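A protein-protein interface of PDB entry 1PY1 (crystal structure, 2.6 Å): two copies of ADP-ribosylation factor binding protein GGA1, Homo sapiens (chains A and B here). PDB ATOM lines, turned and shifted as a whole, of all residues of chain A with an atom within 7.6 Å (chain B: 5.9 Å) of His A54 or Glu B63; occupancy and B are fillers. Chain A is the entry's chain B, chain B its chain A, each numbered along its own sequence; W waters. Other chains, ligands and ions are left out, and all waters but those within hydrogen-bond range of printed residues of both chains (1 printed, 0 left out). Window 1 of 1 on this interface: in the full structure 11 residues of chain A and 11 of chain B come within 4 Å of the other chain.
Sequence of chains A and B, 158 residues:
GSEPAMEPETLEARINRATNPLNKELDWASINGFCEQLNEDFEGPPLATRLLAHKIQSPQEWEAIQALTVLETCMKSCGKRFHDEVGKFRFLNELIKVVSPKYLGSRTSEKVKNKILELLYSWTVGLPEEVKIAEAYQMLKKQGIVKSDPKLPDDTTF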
ATOM      1  N   ASN A  16     -20.281  27.019   3.479  1.00  0.00           N
ATOM      2  CA  ASN A  16     -20.026  27.509   4.824  1.00  0.00           C
ATOM      3  C   ASN A  16     -19.295  28.874   4.823  1.00  0.00           C
ATOM      4  O   ASN A  16     -19.436  29.632   5.746  1.00  0.00           O
ATOM      5  CB  ASN A  16     -19.247  26.489   5.645  1.00  0.00           C
ATOM      6  CG  ASN A  16     -20.076  25.280   5.975  1.00  0.00           C
ATOM      7  OD1 ASN A  16     -21.301  25.330   5.924  1.00  0.00           O
ATOM      8  ND2 ASN A  16     -19.422  24.191   6.326  1.00  0.00           N
ATOM      9  N   ALA A  48     -26.198  20.782  -3.504  1.00  0.00           N
ATOM     10  CA  ALA A  48     -26.256  22.220  -3.321  1.00  0.00           C
ATOM     11  C   ALA A  48     -27.626  22.663  -2.788  1.00  0.00           C
ATOM     12  O   ALA A  48     -27.702  23.376  -1.787  1.00  0.00           O
ATOM     13  CB  ALA A  48     -25.936  22.939  -4.622  1.00  0.00           C
ATOM     14  N   THR A  49     -28.692  22.226  -3.458  1.00  0.00           N
ATOM     15  CA  THR A  49     -30.047  22.592  -3.052  1.00  0.00           C
ATOM     16  C   THR A  49     -30.355  22.129  -1.625  1.00  0.00           C
ATOM     17  O   THR A  49     -31.031  22.823  -0.875  1.00  0.00           O
ATOM     18  CB  THR A  49     -31.080  21.999  -3.986  1.00  0.00           C
ATOM     19  OG1 THR A  49     -30.973  20.569  -3.976  1.00  0.00           O
ATOM     20  CG2 THR A  49     -30.854  22.510  -5.377  1.00  0.00           C
ATOM     21  N   ARG A  50     -29.857  20.951  -1.275  1.00  0.00           N
ATOM     22  CA  ARG A  50     -30.048  20.420   0.063  1.00  0.00           C
ATOM     23  C   ARG A  50     -29.324  21.322   1.096  1.00  0.00           C
ATOM     24  O   ARG A  50     -29.914  21.736   2.107  1.00  0.00           O
ATOM     25  CB  ARG A  50     -29.516  18.986   0.116  1.00  0.00           C
ATOM     26  CG  ARG A  50     -29.227  18.480   1.492  1.00  0.00           C
ATOM     27  CD  ARG A  50     -30.000  17.216   1.771  1.00  0.00           C
ATOM     28  NE  ARG A  50     -29.369  16.016   1.227  1.00  0.00           N
ATOM     29  CZ  ARG A  50     -29.835  14.785   1.434  1.00  0.00           C
ATOM     30  NH1 ARG A  50     -30.930  14.616   2.169  1.00  0.00           N
ATOM     31  NH2 ARG A  50     -29.207  13.727   0.924  1.00  0.00           N
ATOM     32  N   LEU A  51     -28.060  21.632   0.809  1.00  0.00           N
ATOM     33  CA  LEU A  51     -27.257  22.507   1.677  1.00  0.00           C
ATOM     34  C   LEU A  51     -27.842  23.945   1.717  1.00  0.00           C
ATOM     35  O   LEU A  51     -27.791  24.614   2.746  1.00  0.00           O
ATOM     36  CB  LEU A  51     -25.804  22.561   1.190  1.00  0.00           C
ATOM     37  CG  LEU A  51     -24.959  21.303   1.367  1.00  0.00           C
ATOM     38  CD1 LEU A  51     -23.700  21.412   0.544  1.00  0.00           C
ATOM     39  CD2 LEU A  51     -24.626  21.104   2.823  1.00  0.00           C
ATOM     40  N   LEU A  52     -28.391  24.399   0.592  1.00  0.00           N
ATOM     41  CA  LEU A  52     -28.983  25.742   0.541  1.00  0.00           C
ATOM     42  C   LEU A  52     -30.299  25.827   1.371  1.00  0.00           C
ATOM     43  O   LEU A  52     -30.476  26.760   2.160  1.00  0.00           O
ATOM     44  CB  LEU A  52     -29.229  26.174  -0.910  1.00  0.00           C
ATOM     45  CG  LEU A  52     -27.956  26.547  -1.673  1.00  0.00           C
ATOM     46  CD1 LEU A  52     -28.233  26.637  -3.150  1.00  0.00           C
ATOM     47  CD2 LEU A  52     -27.409  27.874  -1.146  1.00  0.00           C
ATOM     48  N   ALA A  53     -31.193  24.854   1.184  1.00  0.00           N
ATOM     49  CA  ALA A  53     -32.463  24.818   1.935  1.00  0.00           C
ATOM     50  C   ALA A  53     -32.184  24.950   3.441  1.00  0.00           C
ATOM     51  O   ALA A  53     -32.866  25.671   4.143  1.00  0.00           O
ATOM     52  CB  ALA A  53     -33.208  23.509   1.667  1.00  0.00           C
ATOM     53  N   HIS A  54     -31.166  24.245   3.920  1.00  0.00           N
ATOM     54  CA  HIS A  54     -30.816  24.346   5.343  1.00  0.00           C
ATOM     55  C   HIS A  54     -30.412  25.806   5.706  1.00  0.00           C
ATOM     56  O   HIS A  54     -31.066  26.425   6.512  1.00  0.00           O
ATOM     57  CB  HIS A  54     -29.687  23.375   5.686  1.00  0.00           C
ATOM     58  CG  HIS A  54     -29.357  23.339   7.142  1.00  0.00           C
ATOM     59  ND1 HIS A  54     -28.168  23.825   7.640  1.00  0.00           N
ATOM     60  CD2 HIS A  54     -30.106  22.987   8.216  1.00  0.00           C
ATOM     61  CE1 HIS A  54     -28.203  23.787   8.962  1.00  0.00           C
ATOM     62  NE2 HIS A  54     -29.368  23.288   9.336  1.00  0.00           N
ATOM     63  N   LYS A  55     -29.363  26.336   5.070  1.00  0.00           N
ATOM     64  CA  LYS A  55     -28.899  27.712   5.328  1.00  0.00           C
ATOM     65  C   LYS A  55     -30.027  28.761   5.205  1.00  0.00           C
ATOM     66  O   LYS A  55     -30.121  29.698   5.993  1.00  0.00           O
ATOM     67  CB  LYS A  55     -27.788  28.099   4.355  1.00  0.00           C
ATOM     68  CG  LYS A  55     -26.580  27.179   4.369  1.00  0.00           C
ATOM     69  CD  LYS A  55     -25.910  27.156   5.737  1.00  0.00           C
ATOM     70  CE  LYS A  55     -24.632  26.311   5.726  1.00  0.00           C
ATOM     71  NZ  LYS A  55     -23.927  26.378   7.029  1.00  0.00           N
ATOM     72  N   ILE A  56     -30.871  28.581   4.198  1.00  0.00           N
ATOM     73  CA  ILE A  56     -31.973  29.497   3.932  1.00  0.00           C
ATOM     74  C   ILE A  56     -32.992  29.509   5.057  1.00  0.00           C
ATOM     75  O   ILE A  56     -33.694  30.504   5.289  1.00  0.00           O
ATOM     76  CB  ILE A  56     -32.628  29.123   2.608  1.00  0.00           C
ATOM     77  CG1 ILE A  56     -31.689  29.551   1.482  1.00  0.00           C
ATOM     78  CG2 ILE A  56     -33.999  29.765   2.460  1.00  0.00           C
ATOM     79  CD1 ILE A  56     -32.167  29.167   0.123  1.00  0.00           C
ATOM     80  N   GLN A  57     -33.030  28.402   5.780  1.00  0.00           N
ATOM     81  CA  GLN A  57     -33.957  28.259   6.897  1.00  0.00           C
ATOM     82  C   GLN A  57     -33.365  28.671   8.250  1.00  0.00           C
ATOM     83  O   GLN A  57     -34.048  28.621   9.258  1.00  0.00           O
ATOM     84  CB  GLN A  57     -34.448  26.809   6.953  1.00  0.00           C
ATOM     85  CG  GLN A  57     -35.264  26.443   5.728  1.00  0.00           C
ATOM     86  CD  GLN A  57     -35.752  25.017   5.736  1.00  0.00           C
ATOM     87  OE1 GLN A  57     -34.983  24.097   5.965  1.00  0.00           O
ATOM     88  NE2 GLN A  57     -37.036  24.828   5.464  1.00  0.00           N
ATOM     89  N   SER A  58     -32.109  29.090   8.263  1.00  0.00           N
ATOM     90  CA  SER A  58     -31.452  29.472   9.541  1.00  0.00           C
ATOM     91  C   SER A  58     -32.121  30.654  10.298  1.00  0.00           C
ATOM     92  O   SER A  58     -32.553  31.613   9.710  1.00  0.00           O
ATOM     93  CB  SER A  58     -29.963  29.798   9.293  1.00  0.00           C
ATOM     94  OG  SER A  58     -29.437  30.637  10.312  1.00  0.00           O
ATOM     95  N   PRO A  59     -32.215  30.546  11.627  1.00  0.00           N
ATOM     96  CA  PRO A  59     -32.817  31.610  12.437  1.00  0.00           C
ATOM     97  C   PRO A  59     -31.987  32.878  12.261  1.00  0.00           C
ATOM     98  O   PRO A  59     -32.500  33.979  12.383  1.00  0.00           O
ATOM     99  CB  PRO A  59     -32.719  31.067  13.861  1.00  0.00           C
ATOM    100  CG  PRO A  59     -32.890  29.601  13.649  1.00  0.00           C
ATOM    101  CD  PRO A  59     -32.005  29.331  12.432  1.00  0.00           C
ATOM    102  N   GLU A  63     -27.454  34.838   7.715  1.00  0.00           N
ATOM    103  CA  GLU A  63     -27.067  33.577   7.180  1.00  0.00           C
ATOM    104  C   GLU A  63     -28.016  33.208   6.032  1.00  0.00           C
ATOM    105  O   GLU A  63     -27.579  32.808   4.972  1.00  0.00           O
ATOM    106  CB  GLU A  63     -27.122  32.524   8.262  1.00  0.00           C
ATOM    107  CG  GLU A  63     -26.844  31.150   7.752  1.00  0.00           C
ATOM    108  CD  GLU A  63     -26.386  30.262   8.849  1.00  0.00           C
ATOM    109  OE1 GLU A  63     -26.942  30.389   9.955  1.00  0.00           O
ATOM    110  OE2 GLU A  63     -25.473  29.450   8.618  1.00  0.00           O
ATOM    111  N   ALA A  64     -29.314  33.373   6.264  1.00  0.00           N
ATOM    112  CA  ALA A  64     -30.323  33.064   5.252  1.00  0.00           C
ATOM    113  C   ALA A  64     -30.256  34.025   4.058  1.00  0.00           C
ATOM    114  O   ALA A  64     -30.423  33.595   2.933  1.00  0.00           O
ATOM    115  CB  ALA A  64     -31.710  33.098   5.870  1.00  0.00           C
ATOM    116  N   ALA A  67     -27.431  32.968   1.992  1.00  0.00           N
ATOM    117  CA  ALA A  67     -27.776  31.707   1.286  1.00  0.00           C
ATOM    118  C   ALA A  67     -28.720  32.042   0.083  1.00  0.00           C
ATOM    119  O   ALA A  67     -28.522  31.557  -1.037  1.00  0.00           O
ATOM    120  CB  ALA A  67     -28.441  30.711   2.230  1.00  0.00           C
ATOM    121  N   PHE A  91     -37.275  20.985  -3.281  1.00  0.00           N
ATOM    122  CA  PHE A  91     -36.603  22.204  -2.857  1.00  0.00           C
ATOM    123  C   PHE A  91     -37.618  23.330  -2.628  1.00  0.00           C
ATOM    124  O   PHE A  91     -37.626  23.928  -1.591  1.00  0.00           O
ATOM    125  CB  PHE A  91     -35.579  22.681  -3.891  1.00  0.00           C
ATOM    126  CG  PHE A  91     -34.889  23.963  -3.506  1.00  0.00           C
ATOM    127  CD1 PHE A  91     -34.051  24.017  -2.398  1.00  0.00           C
ATOM    128  CD2 PHE A  91     -35.125  25.129  -4.207  1.00  0.00           C
ATOM    129  CE1 PHE A  91     -33.468  25.228  -2.001  1.00  0.00           C
ATOM    130  CE2 PHE A  91     -34.547  26.340  -3.818  1.00  0.00           C
ATOM    131  CZ  PHE A  91     -33.723  26.382  -2.716  1.00  0.00           C
ATOM    132  N   GLU A  94     -39.197  23.675   0.885  1.00  0.00           N
ATOM    133  CA  GLU A  94     -38.375  24.299   1.927  1.00  0.00           C
ATOM    134  C   GLU A  94     -38.512  25.862   1.898  1.00  0.00           C
ATOM    135  O   GLU A  94     -38.518  26.506   2.934  1.00  0.00           O
ATOM    136  CB  GLU A  94     -36.917  23.875   1.757  1.00  0.00           C
ATOM    137  CG  GLU A  94     -36.737  22.374   1.731  1.00  0.00           C
ATOM    138  CD  GLU A  94     -37.382  21.695   2.930  1.00  0.00           C
ATOM    139  OE1 GLU A  94     -37.281  22.222   4.046  1.00  0.00           O
ATOM    140  OE2 GLU A  94     -37.981  20.621   2.769  1.00  0.00           O
ATOM    141  N   VAL A  98     -40.531  28.489   4.702  1.00  0.00           N
ATOM    142  CA  VAL A  98     -39.950  29.702   5.241  1.00  0.00           C
ATOM    143  C   VAL A  98     -40.866  30.928   5.153  1.00  0.00           C
ATOM    144  O   VAL A  98     -40.816  31.778   6.020  1.00  0.00           O
ATOM    145  CB  VAL A  98     -38.639  30.012   4.515  1.00  0.00           C
ATOM    146  CG1 VAL A  98     -37.966  31.224   5.118  1.00  0.00           C
ATOM    147  CG2 VAL A  98     -37.749  28.814   4.579  1.00  0.00           C
ATOM    148  N   THR B  19     -20.572  24.334  17.151  1.00  0.00           N
ATOM    149  CA  THR B  19     -21.043  23.359  16.162  1.00  0.00           C
ATOM    150  C   THR B  19     -20.437  23.575  14.774  1.00  0.00           C
ATOM    151  O   THR B  19     -20.968  23.085  13.762  1.00  0.00           O
ATOM    152  CB  THR B  19     -22.554  23.412  16.000  1.00  0.00           C
ATOM    153  OG1 THR B  19     -22.930  24.716  15.553  1.00  0.00           O
ATOM    154  CG2 THR B  19     -23.252  23.087  17.297  1.00  0.00           C
ATOM    155  N   ASN B  20     -19.326  24.305  14.747  1.00  0.00           N
ATOM    156  CA  ASN B  20     -18.627  24.611  13.498  1.00  0.00           C
ATOM    157  C   ASN B  20     -18.093  23.357  12.811  1.00  0.00           C
ATOM    158  O   ASN B  20     -17.379  22.581  13.411  1.00  0.00           O
ATOM    159  CB  ASN B  20     -17.468  25.543  13.782  1.00  0.00           C
ATOM    160  CG  ASN B  20     -16.964  26.216  12.540  1.00  0.00           C
ATOM    161  OD1 ASN B  20     -16.543  25.564  11.588  1.00  0.00           O
ATOM    162  ND2 ASN B  20     -17.010  27.539  12.538  1.00  0.00           N
ATOM    163  N   PRO B  21     -18.444  23.151  11.536  1.00  0.00           N
ATOM    164  CA  PRO B  21     -17.992  21.975  10.772  1.00  0.00           C
ATOM    165  C   PRO B  21     -16.435  21.866  10.607  1.00  0.00           C
ATOM    166  O   PRO B  21     -15.895  20.788  10.357  1.00  0.00           O
ATOM    167  CB  PRO B  21     -18.692  22.154   9.420  1.00  0.00           C
ATOM    168  CG  PRO B  21     -19.946  22.847   9.771  1.00  0.00           C
ATOM    169  CD  PRO B  21     -19.517  23.864  10.821  1.00  0.00           C
ATOM    170  N   HIS B  54     -32.068  23.911  14.675  1.00  0.00           N
ATOM    171  CA  HIS B  54     -31.614  24.180  13.326  1.00  0.00           C
ATOM    172  C   HIS B  54     -30.255  23.490  13.047  1.00  0.00           C
ATOM    173  O   HIS B  54     -30.050  22.926  11.968  1.00  0.00           O
ATOM    174  CB  HIS B  54     -31.512  25.672  13.079  1.00  0.00           C
ATOM    175  CG  HIS B  54     -31.012  26.006  11.714  1.00  0.00           C
ATOM    176  ND1 HIS B  54     -29.764  26.545  11.496  1.00  0.00           N
ATOM    177  CD2 HIS B  54     -31.526  25.746  10.489  1.00  0.00           C
ATOM    178  CE1 HIS B  54     -29.524  26.590  10.200  1.00  0.00           C
ATOM    179  NE2 HIS B  54     -30.576  26.108   9.567  1.00  0.00           N
ATOM    180  N   LYS B  55     -29.342  23.528  14.020  1.00  0.00           N
ATOM    181  CA  LYS B  55     -28.040  22.865  13.843  1.00  0.00           C
ATOM    182  C   LYS B  55     -28.223  21.328  13.791  1.00  0.00           C
ATOM    183  O   LYS B  55     -27.618  20.653  12.957  1.00  0.00           O
ATOM    184  CB  LYS B  55     -27.065  23.233  14.976  1.00  0.00           C
ATOM    185  CG  LYS B  55     -26.629  24.704  15.017  1.00  0.00           C
ATOM    186  CD  LYS B  55     -25.938  25.171  13.725  1.00  0.00           C
ATOM    187  CE  LYS B  55     -25.480  26.643  13.826  1.00  0.00           C
ATOM    188  NZ  LYS B  55     -24.714  27.140  12.636  1.00  0.00           N
ATOM    189  N   ILE B  56     -29.070  20.804  14.672  1.00  0.00           N
ATOM    190  CA  ILE B  56     -29.326  19.368  14.709  1.00  0.00           C
ATOM    191  C   ILE B  56     -29.915  18.822  13.365  1.00  0.00           C
ATOM    192  O   ILE B  56     -29.764  17.654  13.045  1.00  0.00           O
ATOM    193  CB  ILE B  56     -30.281  19.019  15.890  1.00  0.00           C
ATOM    194  CG1 ILE B  56     -29.575  19.270  17.218  1.00  0.00           C
ATOM    195  CG2 ILE B  56     -30.704  17.555  15.841  1.00  0.00           C
ATOM    196  CD1 ILE B  56     -30.437  19.016  18.436  1.00  0.00           C
ATOM    197  N   GLN B  57     -30.551  19.688  12.585  1.00  0.00           N
ATOM    198  CA  GLN B  57     -31.159  19.268  11.300  1.00  0.00           C
ATOM    199  C   GLN B  57     -30.274  19.612  10.101  1.00  0.00           C
ATOM    200  O   GLN B  57     -30.727  19.659   8.961  1.00  0.00           O
ATOM    201  CB  GLN B  57     -32.534  19.933  11.124  1.00  0.00           C
ATOM    202  CG  GLN B  57     -33.408  19.773  12.339  1.00  0.00           C
ATOM    203  CD  GLN B  57     -34.650  20.583  12.272  1.00  0.00           C
ATOM    204  OE1 GLN B  57     -34.645  21.692  11.799  1.00  0.00           O
ATOM    205  NE2 GLN B  57     -35.730  20.032  12.776  1.00  0.00           N
ATOM    206  N   SER B  58     -29.013  19.879  10.391  1.00  0.00           N
ATOM    207  CA  SER B  58     -28.041  20.217   9.357  1.00  0.00           C
ATOM    208  C   SER B  58     -27.652  18.988   8.500  1.00  0.00           C
ATOM    209  O   SER B  58     -27.491  17.898   9.013  1.00  0.00           O
ATOM    210  CB  SER B  58     -26.785  20.795  10.017  1.00  0.00           C
ATOM    211  OG  SER B  58     -25.753  20.904   9.070  1.00  0.00           O
ATOM    212  N   PRO B  59     -27.533  19.165   7.185  1.00  0.00           N
ATOM    213  CA  PRO B  59     -27.157  18.025   6.363  1.00  0.00           C
ATOM    214  C   PRO B  59     -25.702  17.637   6.684  1.00  0.00           C
ATOM    215  O   PRO B  59     -25.273  16.530   6.413  1.00  0.00           O
ATOM    216  CB  PRO B  59     -27.283  18.562   4.941  1.00  0.00           C
ATOM    217  CG  PRO B  59     -28.329  19.543   5.047  1.00  0.00           C
ATOM    218  CD  PRO B  59     -28.010  20.264   6.339  1.00  0.00           C
ATOM    219  N   GLN B  60     -24.960  18.571   7.267  1.00  0.00           N
ATOM    220  CA  GLN B  60     -23.551  18.330   7.585  1.00  0.00           C
ATOM    221  C   GLN B  60     -23.410  17.601   8.929  1.00  0.00           C
ATOM    222  O   GLN B  60     -23.452  18.215   9.984  1.00  0.00           O
ATOM    223  CB  GLN B  60     -22.787  19.674   7.579  1.00  0.00           C
ATOM    224  CG  GLN B  60     -22.882  20.408   6.239  1.00  0.00           C
ATOM    225  CD  GLN B  60     -22.324  21.815   6.269  1.00  0.00           C
ATOM    226  OE1 GLN B  60     -21.205  22.037   6.700  1.00  0.00           O
ATOM    227  NE2 GLN B  60     -23.105  22.773   5.783  1.00  0.00           N
ATOM    228  N   GLU B  61     -23.258  16.281   8.857  1.00  0.00           N
ATOM    229  CA  GLU B  61     -23.153  15.426  10.058  1.00  0.00           C
ATOM    230  C   GLU B  61     -22.337  16.036  11.216  1.00  0.00           C
ATOM    231  O   GLU B  61     -22.854  16.188  12.312  1.00  0.00           O
ATOM    232  CB  GLU B  61     -22.559  14.074   9.691  1.00  0.00           C
ATOM    233  CG  GLU B  61     -22.958  12.950  10.616  1.00  0.00           C
ATOM    234  CD  GLU B  61     -22.277  11.654  10.226  1.00  0.00           C
ATOM    235  OE1 GLU B  61     -22.704  10.568  10.684  1.00  0.00           O
ATOM    236  OE2 GLU B  61     -21.294  11.726   9.450  1.00  0.00           O
ATOM    237  N   TRP B  62     -21.079  16.385  10.971  1.00  0.00           N
ATOM    238  CA  TRP B  62     -20.245  16.948  12.055  1.00  0.00           C
ATOM    239  C   TRP B  62     -20.908  18.162  12.743  1.00  0.00           C
ATOM    240  O   TRP B  62     -20.617  18.445  13.902  1.00  0.00           O
ATOM    241  CB  TRP B  62     -18.858  17.345  11.530  1.00  0.00           C
ATOM    242  CG  TRP B  62     -17.868  17.718  12.611  1.00  0.00           C
ATOM    243  CD1 TRP B  62     -16.972  18.744  12.572  1.00  0.00           C
ATOM    244  CD2 TRP B  62     -17.672  17.072  13.879  1.00  0.00           C
ATOM    245  NE1 TRP B  62     -16.239  18.785  13.732  1.00  0.00           N
ATOM    246  CE2 TRP B  62     -16.651  17.772  14.556  1.00  0.00           C
ATOM    247  CE3 TRP B  62     -18.264  15.972  14.515  1.00  0.00           C
ATOM    248  CZ2 TRP B  62     -16.201  17.416  15.822  1.00  0.00           C
ATOM    249  CZ3 TRP B  62     -17.815  15.607  15.788  1.00  0.00           C
ATOM    250  CH2 TRP B  62     -16.798  16.332  16.428  1.00  0.00           C
ATOM    251  N   GLU B  63     -21.791  18.858  12.013  1.00  0.00           N
ATOM    252  CA  GLU B  63     -22.498  20.039  12.567  1.00  0.00           C
ATOM    253  C   GLU B  63     -23.647  19.627  13.521  1.00  0.00           C
ATOM    254  O   GLU B  63     -23.764  20.144  14.622  1.00  0.00           O
ATOM    255  CB  GLU B  63     -23.047  20.926  11.444  1.00  0.00           C
ATOM    256  CG  GLU B  63     -23.785  22.132  11.974  1.00  0.00           C
ATOM    257  CD  GLU B  63     -23.954  23.234  10.944  1.00  0.00           C
ATOM    258  OE1 GLU B  63     -23.521  24.372  11.212  1.00  0.00           O
ATOM    259  OE2 GLU B  63     -24.514  22.979   9.870  1.00  0.00           O
ATOM    260  N   ALA B  64     -24.465  18.682  13.069  1.00  0.00           N
ATOM    261  CA  ALA B  64     -25.592  18.172  13.849  1.00  0.00           C
ATOM    262  C   ALA B  64     -25.087  17.379  15.073  1.00  0.00           C
ATOM    263  O   ALA B  64     -25.668  17.454  16.153  1.00  0.00           O
ATOM    264  CB  ALA B  64     -26.475  17.280  12.961  1.00  0.00           C
ATOM    265  N   ILE B  65     -24.001  16.628  14.873  1.00  0.00           N
ATOM    266  CA  ILE B  65     -23.401  15.845  15.954  1.00  0.00           C
ATOM    267  C   ILE B  65     -22.886  16.767  17.068  1.00  0.00           C
ATOM    268  O   ILE B  65     -23.199  16.569  18.239  1.00  0.00           O
ATOM    269  CB  ILE B  65     -22.203  14.958  15.473  1.00  0.00           C
ATOM    270  CG1 ILE B  65     -22.671  13.892  14.468  1.00  0.00           C
ATOM    271  CG2 ILE B  65     -21.556  14.268  16.685  1.00  0.00           C
ATOM    272  CD1 ILE B  65     -23.493  12.763  15.092  1.00  0.00           C
ATOM    273  N   GLN B  66     -22.091  17.771  16.703  1.00  0.00           N
ATOM    274  CA  GLN B  66     -21.586  18.672  17.743  1.00  0.00           C
ATOM    275  C   GLN B  66     -22.763  19.338  18.442  1.00  0.00           C
ATOM    276  O   GLN B  66     -22.753  19.522  19.661  1.00  0.00           O
ATOM    277  CB  GLN B  66     -20.657  19.727  17.159  1.00  0.00           C
ATOM    278  CG  GLN B  66     -19.419  19.133  16.525  1.00  0.00           C
ATOM    279  CD  GLN B  66     -18.454  20.188  16.069  1.00  0.00           C
ATOM    280  OE1 GLN B  66     -17.722  20.757  16.866  1.00  0.00           O
ATOM    281  NE2 GLN B  66     -18.467  20.476  14.779  1.00  0.00           N
ATOM    282  N   ALA B  67     -23.780  19.666  17.653  1.00  0.00           N
ATOM    283  CA  ALA B  67     -24.966  20.288  18.200  1.00  0.00           C
ATOM    284  C   ALA B  67     -25.644  19.353  19.220  1.00  0.00           C
ATOM    285  O   ALA B  67     -26.159  19.804  20.214  1.00  0.00           O
ATOM    286  CB  ALA B  67     -25.942  20.655  17.072  1.00  0.00           C
ATOM    287  N   LEU B  68     -25.638  18.052  18.951  1.00  0.00           N
ATOM    288  CA  LEU B  68     -26.241  17.109  19.892  1.00  0.00           C
ATOM    289  C   LEU B  68     -25.394  17.013  21.174  1.00  0.00           C
ATOM    290  O   LEU B  68     -25.917  16.815  22.238  1.00  0.00           O
ATOM    291  CB  LEU B  68     -26.414  15.743  19.234  1.00  0.00           C
ATOM    292  CG  LEU B  68     -27.534  15.732  18.188  1.00  0.00           C
ATOM    293  CD1 LEU B  68     -27.504  14.423  17.416  1.00  0.00           C
ATOM    294  CD2 LEU B  68     -28.891  15.929  18.863  1.00  0.00           C
HETATM  295  O   HOH W   1     -22.881  26.827   9.680  1.00  0.00           O
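NE2 of His A54 sits at hydrogen-bond distance from O of His B54 (2.7 Å).
OE1 of Gln B60 lies within hydrogen-bond range of ND2 of Asn A16 (2.8 Å).
The side-chain amino group (NZ) of Lys B55 is in salt-bridge range of the side-chain carboxylate (OE1) of Glu B63, at 3.3 Å.
OG of Ser B58 lies close to N of Gln B60, 3.1 Å away.
The side-chain hydroxyl (OG) of Ser B58 lies within hydrogen-bond range of the side-chain carboxylate (OE2) of Glu B63.
The side-chain amide oxygen of Asn A16 lies within hydrogen-bond range of the side-chain amino group of Lys A55 (3.0 Å).
The side-chain amino group (NZ) of Lys A55 is in salt-bridge range of the side-chain carboxylate (OE2) of Glu A63 (3.8 Å).
OG of Ser A58 sits at hydrogen-bond distance from OE1 of Glu A63 (2.5 Å).
Among the printed residues, pairs that only touch across the chains: His A54 with Ser B58 (3.3 Å), Ser A58 with His B54 (3.4 Å), His A54 with Pro B59 (3.5 Å), His A54 with Gln B57 (3.5 Å), Pro A59 with His B54 (3.5 Å), Leu A51 with Gln B60 (3.7 Å), Asn A16 with Pro B21 (3.7 Å), Arg A50 with Pro B59 (3.8 Å), Lys A55 with Gln B60 (3.9 Å) and His A54 with Glu B63 (3.9 Å).
Of the printed residues of chain A, Glu B63 touches His A54 (3.9 Å).
Of the printed residues of chain B, Lys A55 touches Gln B60 (3.9 Å).
Of the printed residues of chain A, Pro B59 touches Arg A50 (3.8 Å) and His A54 (3.5 Å).
Gln B66 touches none of the printed residues of chain A.
The nearest residue of chain B that does not touch His A54 is Lys B55 (4.7 Å).
The nearest printed residue of chain A that does not touch Pro B59 is Leu A51 (4.2 Å).
Of the 19 printed residues of chain A, 7 touch a printed residue of chain B.
Hydrophobic or aromatic side chains of chain A within 4 Å of the printed part of chain B: Leu A51, His A54 and Pro A59.
Of the 18 printed residues of chain B, 7 touch a printed residue of chain A.
Along chain B the printed residues that touch a printed residue of chain A span positions 21 to 63.
Among the printed residues, 12 pairs touch across the chains.
His B54 touches its own counterpart, His A54.
His A54 touches Gln B57, but with the chains exchanged Gln A57 does not touch His B54 (4.01 Å).
His A54 touches Pro B59, and with the chains exchanged Pro A59 touches His B54.
His A54 touches Glu B63, but with the chains exchanged Glu A63 does not touch His B54 (4.6 Å).
Of the 12 pairs that touch across the chains among the printed residues, 5 have their exchanged pair printed and touching as well.
Water W1 lies within hydrogen-bond range of NZ of Lys A55, OE1 of Glu B63 and NZ of Lys B55.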
